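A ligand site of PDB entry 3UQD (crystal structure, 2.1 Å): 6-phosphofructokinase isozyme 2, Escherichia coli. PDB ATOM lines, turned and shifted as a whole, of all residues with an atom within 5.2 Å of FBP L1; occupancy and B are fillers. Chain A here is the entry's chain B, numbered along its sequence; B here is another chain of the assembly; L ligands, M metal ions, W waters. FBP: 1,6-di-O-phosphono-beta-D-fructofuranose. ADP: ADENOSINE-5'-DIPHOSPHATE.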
ATOM      1  N   ALA A  10      -9.607 -20.876   0.094  1.00  0.00           N
ATOM      2  CA  ALA A  10      -9.379 -20.680   1.532  1.00  0.00           C
ATOM      3  C   ALA A  10      -9.922 -19.338   2.024  1.00  0.00           C
ATOM      4  O   ALA A  10      -9.172 -18.409   2.265  1.00  0.00           O
ATOM      5  CB  ALA A  10      -7.896 -20.809   1.854  1.00  0.00           C
ATOM      6  N   SER A  12     -11.933 -16.443   4.472  1.00  0.00           N
ATOM      7  CA  SER A  12     -11.617 -15.992   5.814  1.00  0.00           C
ATOM      8  C   SER A  12     -12.683 -15.030   6.351  1.00  0.00           C
ATOM      9  O   SER A  12     -13.186 -14.191   5.615  1.00  0.00           O
ATOM     10  CB  SER A  12     -10.246 -15.327   5.845  1.00  0.00           C
ATOM     11  OG  SER A  12      -9.979 -14.736   7.101  1.00  0.00           O
ATOM     12  N   ASP A  14     -12.496 -12.116   8.513  1.00  0.00           N
ATOM     13  CA  ASP A  14     -11.509 -11.238   9.116  1.00  0.00           C
ATOM     14  C   ASP A  14     -12.097 -10.533  10.336  1.00  0.00           C
ATOM     15  O   ASP A  14     -13.274 -10.172  10.359  1.00  0.00           O
ATOM     16  CB  ASP A  14     -10.980 -10.230   8.096  1.00  0.00           C
ATOM     17  CG  ASP A  14     -10.218 -10.891   6.960  1.00  0.00           C
ATOM     18  OD1 ASP A  14      -9.828 -12.072   7.111  1.00  0.00           O
ATOM     19  OD2 ASP A  14     -10.009 -10.231   5.919  1.00  0.00           O
ATOM     20  N   PRO A  37     -15.816  -9.820   5.489  1.00  0.00           N
ATOM     21  CA  PRO A  37     -15.424 -10.967   4.671  1.00  0.00           C
ATOM     22  C   PRO A  37     -13.967 -10.844   4.235  1.00  0.00           C
ATOM     23  O   PRO A  37     -13.521  -9.740   3.966  1.00  0.00           O
ATOM     24  CB  PRO A  37     -16.331 -10.852   3.447  1.00  0.00           C
ATOM     25  CG  PRO A  37     -17.471 -10.015   3.885  1.00  0.00           C
ATOM     26  CD  PRO A  37     -16.890  -9.032   4.846  1.00  0.00           C
ATOM     27  N   GLY A  38     -13.249 -11.962   4.180  1.00  0.00           N
ATOM     28  CA  GLY A  38     -11.865 -11.950   3.759  1.00  0.00           C
ATOM     29  C   GLY A  38     -11.517 -13.128   2.872  1.00  0.00           C
ATOM     30  O   GLY A  38     -12.370 -13.968   2.582  1.00  0.00           O
ATOM     31  N   GLY A  39     -10.260 -13.197   2.442  1.00  0.00           N
ATOM     32  CA  GLY A  39      -9.857 -14.199   1.471  1.00  0.00           C
ATOM     33  C   GLY A  39      -9.718 -13.566   0.100  1.00  0.00           C
ATOM     34  O   GLY A  39     -10.481 -12.665  -0.245  1.00  0.00           O
ATOM     35  N   GLY A  40      -8.739 -14.022  -0.666  1.00  0.00           N
ATOM     36  CA  GLY A  40      -8.345 -13.398  -1.916  1.00  0.00           C
ATOM     37  C   GLY A  40      -9.455 -13.096  -2.911  1.00  0.00           C
ATOM     38  O   GLY A  40      -9.749 -11.918  -3.188  1.00  0.00           O
ATOM     39  N   ASN A  43     -12.294 -10.861  -1.543  1.00  0.00           N
ATOM     40  CA  ASN A  43     -11.997  -9.423  -1.554  1.00  0.00           C
ATOM     41  C   ASN A  43     -12.051  -8.838  -2.972  1.00  0.00           C
ATOM     42  O   ASN A  43     -12.499  -7.705  -3.171  1.00  0.00           O
ATOM     43  CB  ASN A  43     -10.652  -9.127  -0.894  1.00  0.00           C
ATOM     44  CG  ASN A  43     -10.650  -9.404   0.607  1.00  0.00           C
ATOM     45  OD1 ASN A  43     -11.691  -9.356   1.251  1.00  0.00           O
ATOM     46  ND2 ASN A  43      -9.483  -9.703   1.145  1.00  0.00           N
ATOM     47  N   ARG A  90     -12.061 -20.315   8.606  1.00  0.00           N
ATOM     48  CA  ARG A  90     -11.077 -19.771   9.533  1.00  0.00           C
ATOM     49  C   ARG A  90     -11.437 -18.356   9.953  1.00  0.00           C
ATOM     50  O   ARG A  90     -12.311 -17.714   9.352  1.00  0.00           O
ATOM     51  CB  ARG A  90      -9.673 -19.800   8.933  1.00  0.00           C
ATOM     52  CG  ARG A  90      -9.493 -18.880   7.731  1.00  0.00           C
ATOM     53  CD  ARG A  90      -8.041 -18.842   7.265  1.00  0.00           C
ATOM     54  NE  ARG A  90      -7.936 -18.399   5.883  1.00  0.00           N
ATOM     55  CZ  ARG A  90      -6.792 -18.095   5.271  1.00  0.00           C
ATOM     56  NH1 ARG A  90      -5.649 -18.175   5.938  1.00  0.00           N
ATOM     57  NH2 ARG A  90      -6.801 -17.708   4.008  1.00  0.00           N
ATOM     58  N   ASN A  92      -9.263 -14.926  10.989  1.00  0.00           N
ATOM     59  CA  ASN A  92      -8.001 -14.239  11.189  1.00  0.00           C
ATOM     60  C   ASN A  92      -8.166 -12.951  11.999  1.00  0.00           C
ATOM     61  O   ASN A  92      -9.189 -12.280  11.881  1.00  0.00           O
ATOM     62  CB  ASN A  92      -7.340 -13.934   9.838  1.00  0.00           C
ATOM     63  CG  ASN A  92      -7.083 -15.189   9.024  1.00  0.00           C
ATOM     64  OD1 ASN A  92      -7.043 -16.289   9.565  1.00  0.00           O
ATOM     65  ND2 ASN A  92      -6.907 -15.024   7.723  1.00  0.00           N
ATOM     66  N   HIS A  94      -6.692  -9.194  13.004  1.00  0.00           N
ATOM     67  CA  HIS A  94      -5.794  -8.093  12.647  1.00  0.00           C
ATOM     68  C   HIS A  94      -5.794  -7.063  13.767  1.00  0.00           C
ATOM     69  O   HIS A  94      -6.849  -6.528  14.122  1.00  0.00           O
ATOM     70  CB  HIS A  94      -6.215  -7.462  11.320  1.00  0.00           C
ATOM     71  CG  HIS A  94      -6.206  -8.421  10.174  1.00  0.00           C
ATOM     72  ND1 HIS A  94      -7.145  -8.389   9.162  1.00  0.00           N
ATOM     73  CD2 HIS A  94      -5.372  -9.445   9.881  1.00  0.00           C
ATOM     74  CE1 HIS A  94      -6.880  -9.351   8.299  1.00  0.00           C
ATOM     75  NE2 HIS A  94      -5.812 -10.002   8.705  1.00  0.00           N
ATOM     76  N   ARG A 105      -0.884  -9.108  11.968  1.00  0.00           N
ATOM     77  CA  ARG A 105      -1.841  -9.971  11.286  1.00  0.00           C
ATOM     78  C   ARG A 105      -1.617 -11.438  11.601  1.00  0.00           C
ATOM     79  O   ARG A 105      -0.666 -12.051  11.115  1.00  0.00           O
ATOM     80  CB  ARG A 105      -1.755  -9.749   9.779  1.00  0.00           C
ATOM     81  CG  ARG A 105      -1.931  -8.309   9.347  1.00  0.00           C
ATOM     82  CD  ARG A 105      -1.857  -8.201   7.837  1.00  0.00           C
ATOM     83  NE  ARG A 105      -2.818  -9.086   7.190  1.00  0.00           N
ATOM     84  CZ  ARG A 105      -2.877  -9.303   5.884  1.00  0.00           C
ATOM     85  NH1 ARG A 105      -2.030  -8.682   5.063  1.00  0.00           N
ATOM     86  NH2 ARG A 105      -3.781 -10.133   5.392  1.00  0.00           N
ATOM     87  N   VAL A 107      -2.686 -15.075  11.024  1.00  0.00           N
ATOM     88  CA  VAL A 107      -3.401 -15.775   9.959  1.00  0.00           C
ATOM     89  C   VAL A 107      -3.476 -17.287  10.190  1.00  0.00           C
ATOM     90  O   VAL A 107      -2.471 -18.009  10.080  1.00  0.00           O
ATOM     91  CB  VAL A 107      -2.756 -15.487   8.587  1.00  0.00           C
ATOM     92  CG1 VAL A 107      -3.567 -16.152   7.478  1.00  0.00           C
ATOM     93  CG2 VAL A 107      -2.674 -13.992   8.355  1.00  0.00           C
ATOM     94  N   GLY A 138      -5.967 -16.224  -3.624  1.00  0.00           N
ATOM     95  CA  GLY A 138      -5.869 -16.616  -2.231  1.00  0.00           C
ATOM     96  C   GLY A 138      -5.032 -17.875  -2.056  1.00  0.00           C
ATOM     97  O   GLY A 138      -4.714 -18.557  -3.027  1.00  0.00           O
ATOM     98  N   SER A 139      -4.679 -18.183  -0.808  1.00  0.00           N
ATOM     99  CA  SER A 139      -3.833 -19.328  -0.517  1.00  0.00           C
ATOM    100  C   SER A 139      -4.567 -20.637  -0.763  1.00  0.00           C
ATOM    101  O   SER A 139      -5.783 -20.660  -0.932  1.00  0.00           O
ATOM    102  CB  SER A 139      -3.322 -19.273   0.931  1.00  0.00           C
ATOM    103  OG  SER A 139      -4.407 -19.215   1.833  1.00  0.00           O
ATOM    104  N   THR A 251      -3.146  -2.293   4.721  1.00  0.00           N
ATOM    105  CA  THR A 251      -2.871  -2.715   3.356  1.00  0.00           C
ATOM    106  C   THR A 251      -3.634  -3.993   3.021  1.00  0.00           C
ATOM    107  O   THR A 251      -3.558  -4.508   1.904  1.00  0.00           O
ATOM    108  CB  THR A 251      -1.351  -2.929   3.141  1.00  0.00           C
ATOM    109  OG1 THR A 251      -0.624  -1.821   3.701  1.00  0.00           O
ATOM    110  CG2 THR A 251      -1.006  -3.046   1.668  1.00  0.00           C
ATOM    111  N   VAL A 252      -4.379  -4.512   3.995  1.00  0.00           N
ATOM    112  CA  VAL A 252      -5.105  -5.765   3.807  1.00  0.00           C
ATOM    113  C   VAL A 252      -6.123  -5.656   2.667  1.00  0.00           C
ATOM    114  O   VAL A 252      -7.071  -4.869   2.740  1.00  0.00           O
ATOM    115  CB  VAL A 252      -5.807  -6.234   5.099  1.00  0.00           C
ATOM    116  CG1 VAL A 252      -6.543  -7.550   4.861  1.00  0.00           C
ATOM    117  CG2 VAL A 252      -4.801  -6.384   6.224  1.00  0.00           C
ATOM    118  N   GLY A 253      -5.923  -6.443   1.621  1.00  0.00           N
ATOM    119  CA  GLY A 253      -6.828  -6.448   0.479  1.00  0.00           C
ATOM    120  C   GLY A 253      -6.489  -5.406  -0.565  1.00  0.00           C
ATOM    121  O   GLY A 253      -7.238  -5.230  -1.533  1.00  0.00           O
ATOM    122  N   ALA A 254      -5.378  -4.698  -0.377  1.00  0.00           N
ATOM    123  CA  ALA A 254      -4.946  -3.706  -1.364  1.00  0.00           C
ATOM    124  C   ALA A 254      -4.691  -4.380  -2.714  1.00  0.00           C
ATOM    125  O   ALA A 254      -5.200  -3.941  -3.738  1.00  0.00           O
ATOM    126  CB  ALA A 254      -3.690  -2.992  -0.880  1.00  0.00           C
ATOM    127  N   GLY A 255      -3.924  -5.455  -2.686  1.00  0.00           N
ATOM    128  CA  GLY A 255      -3.674  -6.255  -3.877  1.00  0.00           C
ATOM    129  C   GLY A 255      -4.949  -6.785  -4.511  1.00  0.00           C
ATOM    130  O   GLY A 255      -5.102  -6.770  -5.721  1.00  0.00           O
ATOM    131  N   ASP A 256      -5.883  -7.241  -3.674  1.00  0.00           N
ATOM    132  CA  ASP A 256      -7.149  -7.767  -4.188  1.00  0.00           C
ATOM    133  C   ASP A 256      -8.015  -6.686  -4.834  1.00  0.00           C
ATOM    134  O   ASP A 256      -8.621  -6.903  -5.891  1.00  0.00           O
ATOM    135  CB  ASP A 256      -7.923  -8.486  -3.076  1.00  0.00           C
ATOM    136  CG  ASP A 256      -7.102  -9.577  -2.421  1.00  0.00           C
ATOM    137  OD1 ASP A 256      -6.426 -10.336  -3.144  1.00  0.00           O
ATOM    138  OD2 ASP A 256      -7.140  -9.685  -1.175  1.00  0.00           O
ATOM    139  N   THR A 292     -10.305  -4.439   6.785  1.00  0.00           N
ATOM    140  CA  THR A 292     -10.452  -4.953   5.432  1.00  0.00           C
ATOM    141  C   THR A 292     -11.641  -4.301   4.742  1.00  0.00           C
ATOM    142  O   THR A 292     -12.505  -4.980   4.195  1.00  0.00           O
ATOM    143  CB  THR A 292     -10.673  -6.487   5.436  1.00  0.00           C
ATOM    144  OG1 THR A 292      -9.947  -7.092   6.514  1.00  0.00           O
ATOM    145  CG2 THR A 292     -10.237  -7.118   4.113  1.00  0.00           C
ATOM    146  N   LYS B  27       1.910 -11.163   6.824  1.00  0.00           N
ATOM    147  CA  LYS B  27       1.031 -12.247   7.244  1.00  0.00           C
ATOM    148  C   LYS B  27       1.788 -13.213   8.140  1.00  0.00           C
ATOM    149  O   LYS B  27       2.681 -13.927   7.682  1.00  0.00           O
ATOM    150  CB  LYS B  27       0.459 -13.002   6.042  1.00  0.00           C
ATOM    151  CG  LYS B  27      -0.631 -12.245   5.292  1.00  0.00           C
ATOM    152  CD  LYS B  27      -1.142 -13.046   4.100  1.00  0.00           C
ATOM    153  CE  LYS B  27      -2.174 -12.261   3.320  1.00  0.00           C
ATOM    154  NZ  LYS B  27      -2.503 -12.870   1.988  1.00  0.00           N
ATOM    155  N   ARG B  29       1.841 -16.509   9.808  1.00  0.00           N
ATOM    156  CA  ARG B  29       1.169 -17.816   9.722  1.00  0.00           C
ATOM    157  C   ARG B  29       1.050 -18.483  11.091  1.00  0.00           C
ATOM    158  O   ARG B  29       2.048 -18.779  11.738  1.00  0.00           O
ATOM    159  CB  ARG B  29       1.896 -18.733   8.722  1.00  0.00           C
ATOM    160  CG  ARG B  29       1.343 -18.725   7.300  1.00  0.00           C
ATOM    161  CD  ARG B  29       1.192 -17.313   6.731  1.00  0.00           C
ATOM    162  NE  ARG B  29       0.940 -17.303   5.293  1.00  0.00           N
ATOM    163  CZ  ARG B  29      -0.267 -17.324   4.740  1.00  0.00           C
ATOM    164  NH1 ARG B  29      -1.360 -17.372   5.505  1.00  0.00           N
ATOM    165  NH2 ARG B  29      -0.405 -17.304   3.423  1.00  0.00           N
HETATM  166  P1  FBP L   1      -3.604  -9.434   1.442  1.00  0.00           P
HETATM  167  O1P FBP L   1      -2.707 -10.365   0.539  1.00  0.00           O
HETATM  168  O2P FBP L   1      -3.033  -9.226   2.813  1.00  0.00           O
HETATM  169  O3P FBP L   1      -3.788  -8.113   0.745  1.00  0.00           O
HETATM  170  O1  FBP L   1      -5.000 -10.187   1.403  1.00  0.00           O
HETATM  171  C1  FBP L   1      -5.934 -10.108   2.461  1.00  0.00           C
HETATM  172  C2  FBP L   1      -6.493 -11.425   2.907  1.00  0.00           C
HETATM  173  O2  FBP L   1      -7.182 -12.000   1.830  1.00  0.00           O
HETATM  174  C3  FBP L   1      -7.301 -11.340   4.114  1.00  0.00           C
HETATM  175  O3  FBP L   1      -8.603 -11.013   3.789  1.00  0.00           O
HETATM  176  C4  FBP L   1      -7.195 -12.680   4.631  1.00  0.00           C
HETATM  177  O4  FBP L   1      -7.356 -12.629   6.022  1.00  0.00           O
HETATM  178  C5  FBP L   1      -5.850 -13.077   4.293  1.00  0.00           C
HETATM  179  O5  FBP L   1      -5.427 -12.243   3.217  1.00  0.00           O
HETATM  180  C6  FBP L   1      -5.737 -14.472   3.822  1.00  0.00           C
HETATM  181  O6  FBP L   1      -4.451 -14.837   3.390  1.00  0.00           O
HETATM  182  P2  FBP L   1      -4.155 -16.185   2.635  1.00  0.00           P
HETATM  183  O4P FBP L   1      -2.714 -16.077   1.994  1.00  0.00           O
HETATM  184  O5P FBP L   1      -5.154 -16.303   1.501  1.00  0.00           O
HETATM  185  O6P FBP L   1      -4.228 -17.369   3.583  1.00  0.00           O
HETATM  186  PB  ADP L   2       0.644  -7.378  -2.304  1.00  0.00           P
HETATM  187  O1B ADP L   2       2.135  -7.309  -2.112  1.00  0.00           O
HETATM  188  O2B ADP L   2       0.176  -8.393  -3.313  1.00  0.00           O
HETATM  189  O3B ADP L   2      -0.087  -7.412  -0.983  1.00  0.00           O
HETATM  190  PA  ADP L   2       1.101  -4.647  -2.875  1.00  0.00           P
HETATM  191  O1A ADP L   2       2.000  -4.632  -4.091  1.00  0.00           O
HETATM  192  O2A ADP L   2       1.739  -4.532  -1.510  1.00  0.00           O
HETATM  193  O3A ADP L   2       0.205  -5.978  -2.935  1.00  0.00           O
HETATM  194  O5' ADP L   2      -0.034  -3.516  -3.059  1.00  0.00           O
HETATM  195  C5' ADP L   2      -0.895  -3.548  -4.190  1.00  0.00           C
HETATM  196  C4' ADP L   2      -1.313  -2.136  -4.531  1.00  0.00           C
HETATM  197  O4' ADP L   2      -1.834  -1.478  -3.373  1.00  0.00           O
HETATM  198  C3' ADP L   2      -0.100  -1.309  -4.934  1.00  0.00           C
HETATM  199  O3' ADP L   2       0.227  -1.438  -6.308  1.00  0.00           O
HETATM  200  C2' ADP L   2      -0.551   0.096  -4.587  1.00  0.00           C
HETATM  201  O2' ADP L   2      -1.402   0.583  -5.626  1.00  0.00           O
HETATM  202  C1' ADP L   2      -1.391  -0.119  -3.344  1.00  0.00           C
HETATM  203  N9  ADP L   2      -0.520   0.086  -2.166  1.00  0.00           N
HETATM  204  C8  ADP L   2      -0.034  -0.896  -1.377  1.00  0.00           C
HETATM  205  N7  ADP L   2       0.721  -0.368  -0.375  1.00  0.00           N
HETATM  206  C5  ADP L   2       0.730   0.971  -0.536  1.00  0.00           C
HETATM  207  C6  ADP L   2       1.335   2.127   0.173  1.00  0.00           C
HETATM  208  N6  ADP L   2       2.100   1.944   1.267  1.00  0.00           N
HETATM  209  N1  ADP L   2       1.086   3.360  -0.311  1.00  0.00           N
HETATM  210  C2  ADP L   2       0.335   3.554  -1.406  1.00  0.00           C
HETATM  211  N3  ADP L   2      -0.245   2.552  -2.097  1.00  0.00           N
HETATM  212  C4  ADP L   2      -0.081   1.264  -1.717  1.00  0.00           C
HETATM  213 MG    MG M   1      -0.819 -10.948  -2.659  1.00  0.00          MG
HETATM  214  O   HOH W   1      -5.740 -13.401   0.120  1.00  0.00           O
HETATM  215  O   HOH W   2      -2.424  -6.395  -0.349  1.00  0.00           O
HETATM  216  O   HOH W   3      -7.650 -16.485   0.581  1.00  0.00           O
HETATM  217  O   HOH W   4      -1.325  -6.299   2.521  1.00  0.00           O
HETATM  218  O   HOH W   5      -4.940 -11.592   6.907  1.00  0.00           O
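An oxygen (O1) of FBP L1 lies close to the side-chain carboxylate of Asp 256 (3.4 Å). Ser 12 touches FBP L1. CA of Gly 38 touches O3 of FBP L1, 3.4 Å away. Gly 40 touches FBP L1 (N to O2, 3.6 Å). CA of Gly 138 touches O5P of FBP L1, at 3.8 Å. Thr 251 touches FBP L1. Val 252 touches FBP L1. N of Ala 254 touches O3P of FBP L1, at 3.9 Å. Hydrophobic or aromatic side chains that line FBP L1: Val 252. Within 4 Å of FBP L1: Ser 12, Asp 14, Gly 38, Gly 39, Gly 40, Asn 43, Arg 90, Asn 92, Arg 105, Gly 138, Ser 139, Thr 251, Val 252, Gly 253, Ala 254, Asp 256, Lys 27 of chain B and Arg 29 of chain B.
Water W2 lies within hydrogen-bond range of an oxygen (O3P) of FBP L1, an oxygen (O3B) of ADP L2, the backbone NH (N) of Gly 255, the backbone carbonyl oxygen (O) of Thr 251 and the backbone NH (N) of Ala 254. Water W1 bridges an oxygen (O2) of FBP L1 (2.6 Å) and the backbone NH (N) of Gly 40 (3.2 Å). Water W3 lies within hydrogen-bond range of O5P of FBP L1 (2.7 Å), N of Gly 40 (3.0 Å) and O of Ala 10 (3.0 Å). Water W5 lies within hydrogen-bond range of the guanidinium group of Arg 105, a ring nitrogen (NE2) of His 94 and an oxygen (O4) of FBP L1. Water W4 bridges O of Thr 251 and O2P of FBP L1.
The guanidinium group (NH1) of Arg 105 lies within salt-bridge range of an oxygen (O2P) of FBP L1, 2.5 Å away. N of Ser 139 lies within hydrogen-bond range of O5P of FBP L1 (3.0 Å). The side-chain hydroxyl of Ser 139 lies within hydrogen-bond range of an oxygen (O6P) of FBP L1 (2.5 Å). NH2 of Arg 90 lies within salt-bridge range of O6P of FBP L1. An oxygen (O3) of FBP L1 lies within hydrogen-bond range of the side-chain carboxylate (OD2) of Asp 14, 2.7 Å away. The backbone NH (N) of Gly 253 sits at hydrogen-bond distance from an oxygen (O3P) of FBP L1 (2.8 Å). The side-chain amino group of Lys 27 of chain B lies within salt-bridge range of an oxygen (O1P) of FBP L1 (2.9 Å). ND2 of Asn 92 lies within hydrogen-bond range of O4 of FBP L1. NH2 of Arg 29 of chain B is in salt-bridge range of O4P of FBP L1 (3.0 Å). The backbone NH (N) of Gly 39 sits at hydrogen-bond distance from an oxygen (O3) of FBP L1 (3.1 Å). O3 of FBP L1 lies within hydrogen-bond range of ND2 of Asn 43 (3.1 Å).
NE of Arg 105 is in hydrogen-bond range of NE2 of His 94, at 3.5 Å. O of Ala 10 lies within hydrogen-bond range of NH2 of Arg 90 (3.0 Å). OD1 of Asp 14 sits at hydrogen-bond distance from OG of Ser 12 (2.7 Å). The side-chain hydroxyl (OG) of Ser 12 sits at hydrogen-bond distance from the side-chain amide nitrogen (ND2) of Asn 92. The side-chain amide nitrogen (ND2) of Asn 43 sits close to the backbone carbonyl oxygen (O) of Gly 39, 3.4 Å away. ND2 of Asn 43 is in hydrogen-bond range of OD2 of Asp 256 (3.3 Å). The backbone carbonyl oxygen of Pro 37 sits close to the side-chain amide oxygen of Asn 43, 3.3 Å away. N of Gly 38 is in hydrogen-bond range of O of Ser 12, 2.7 Å away.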
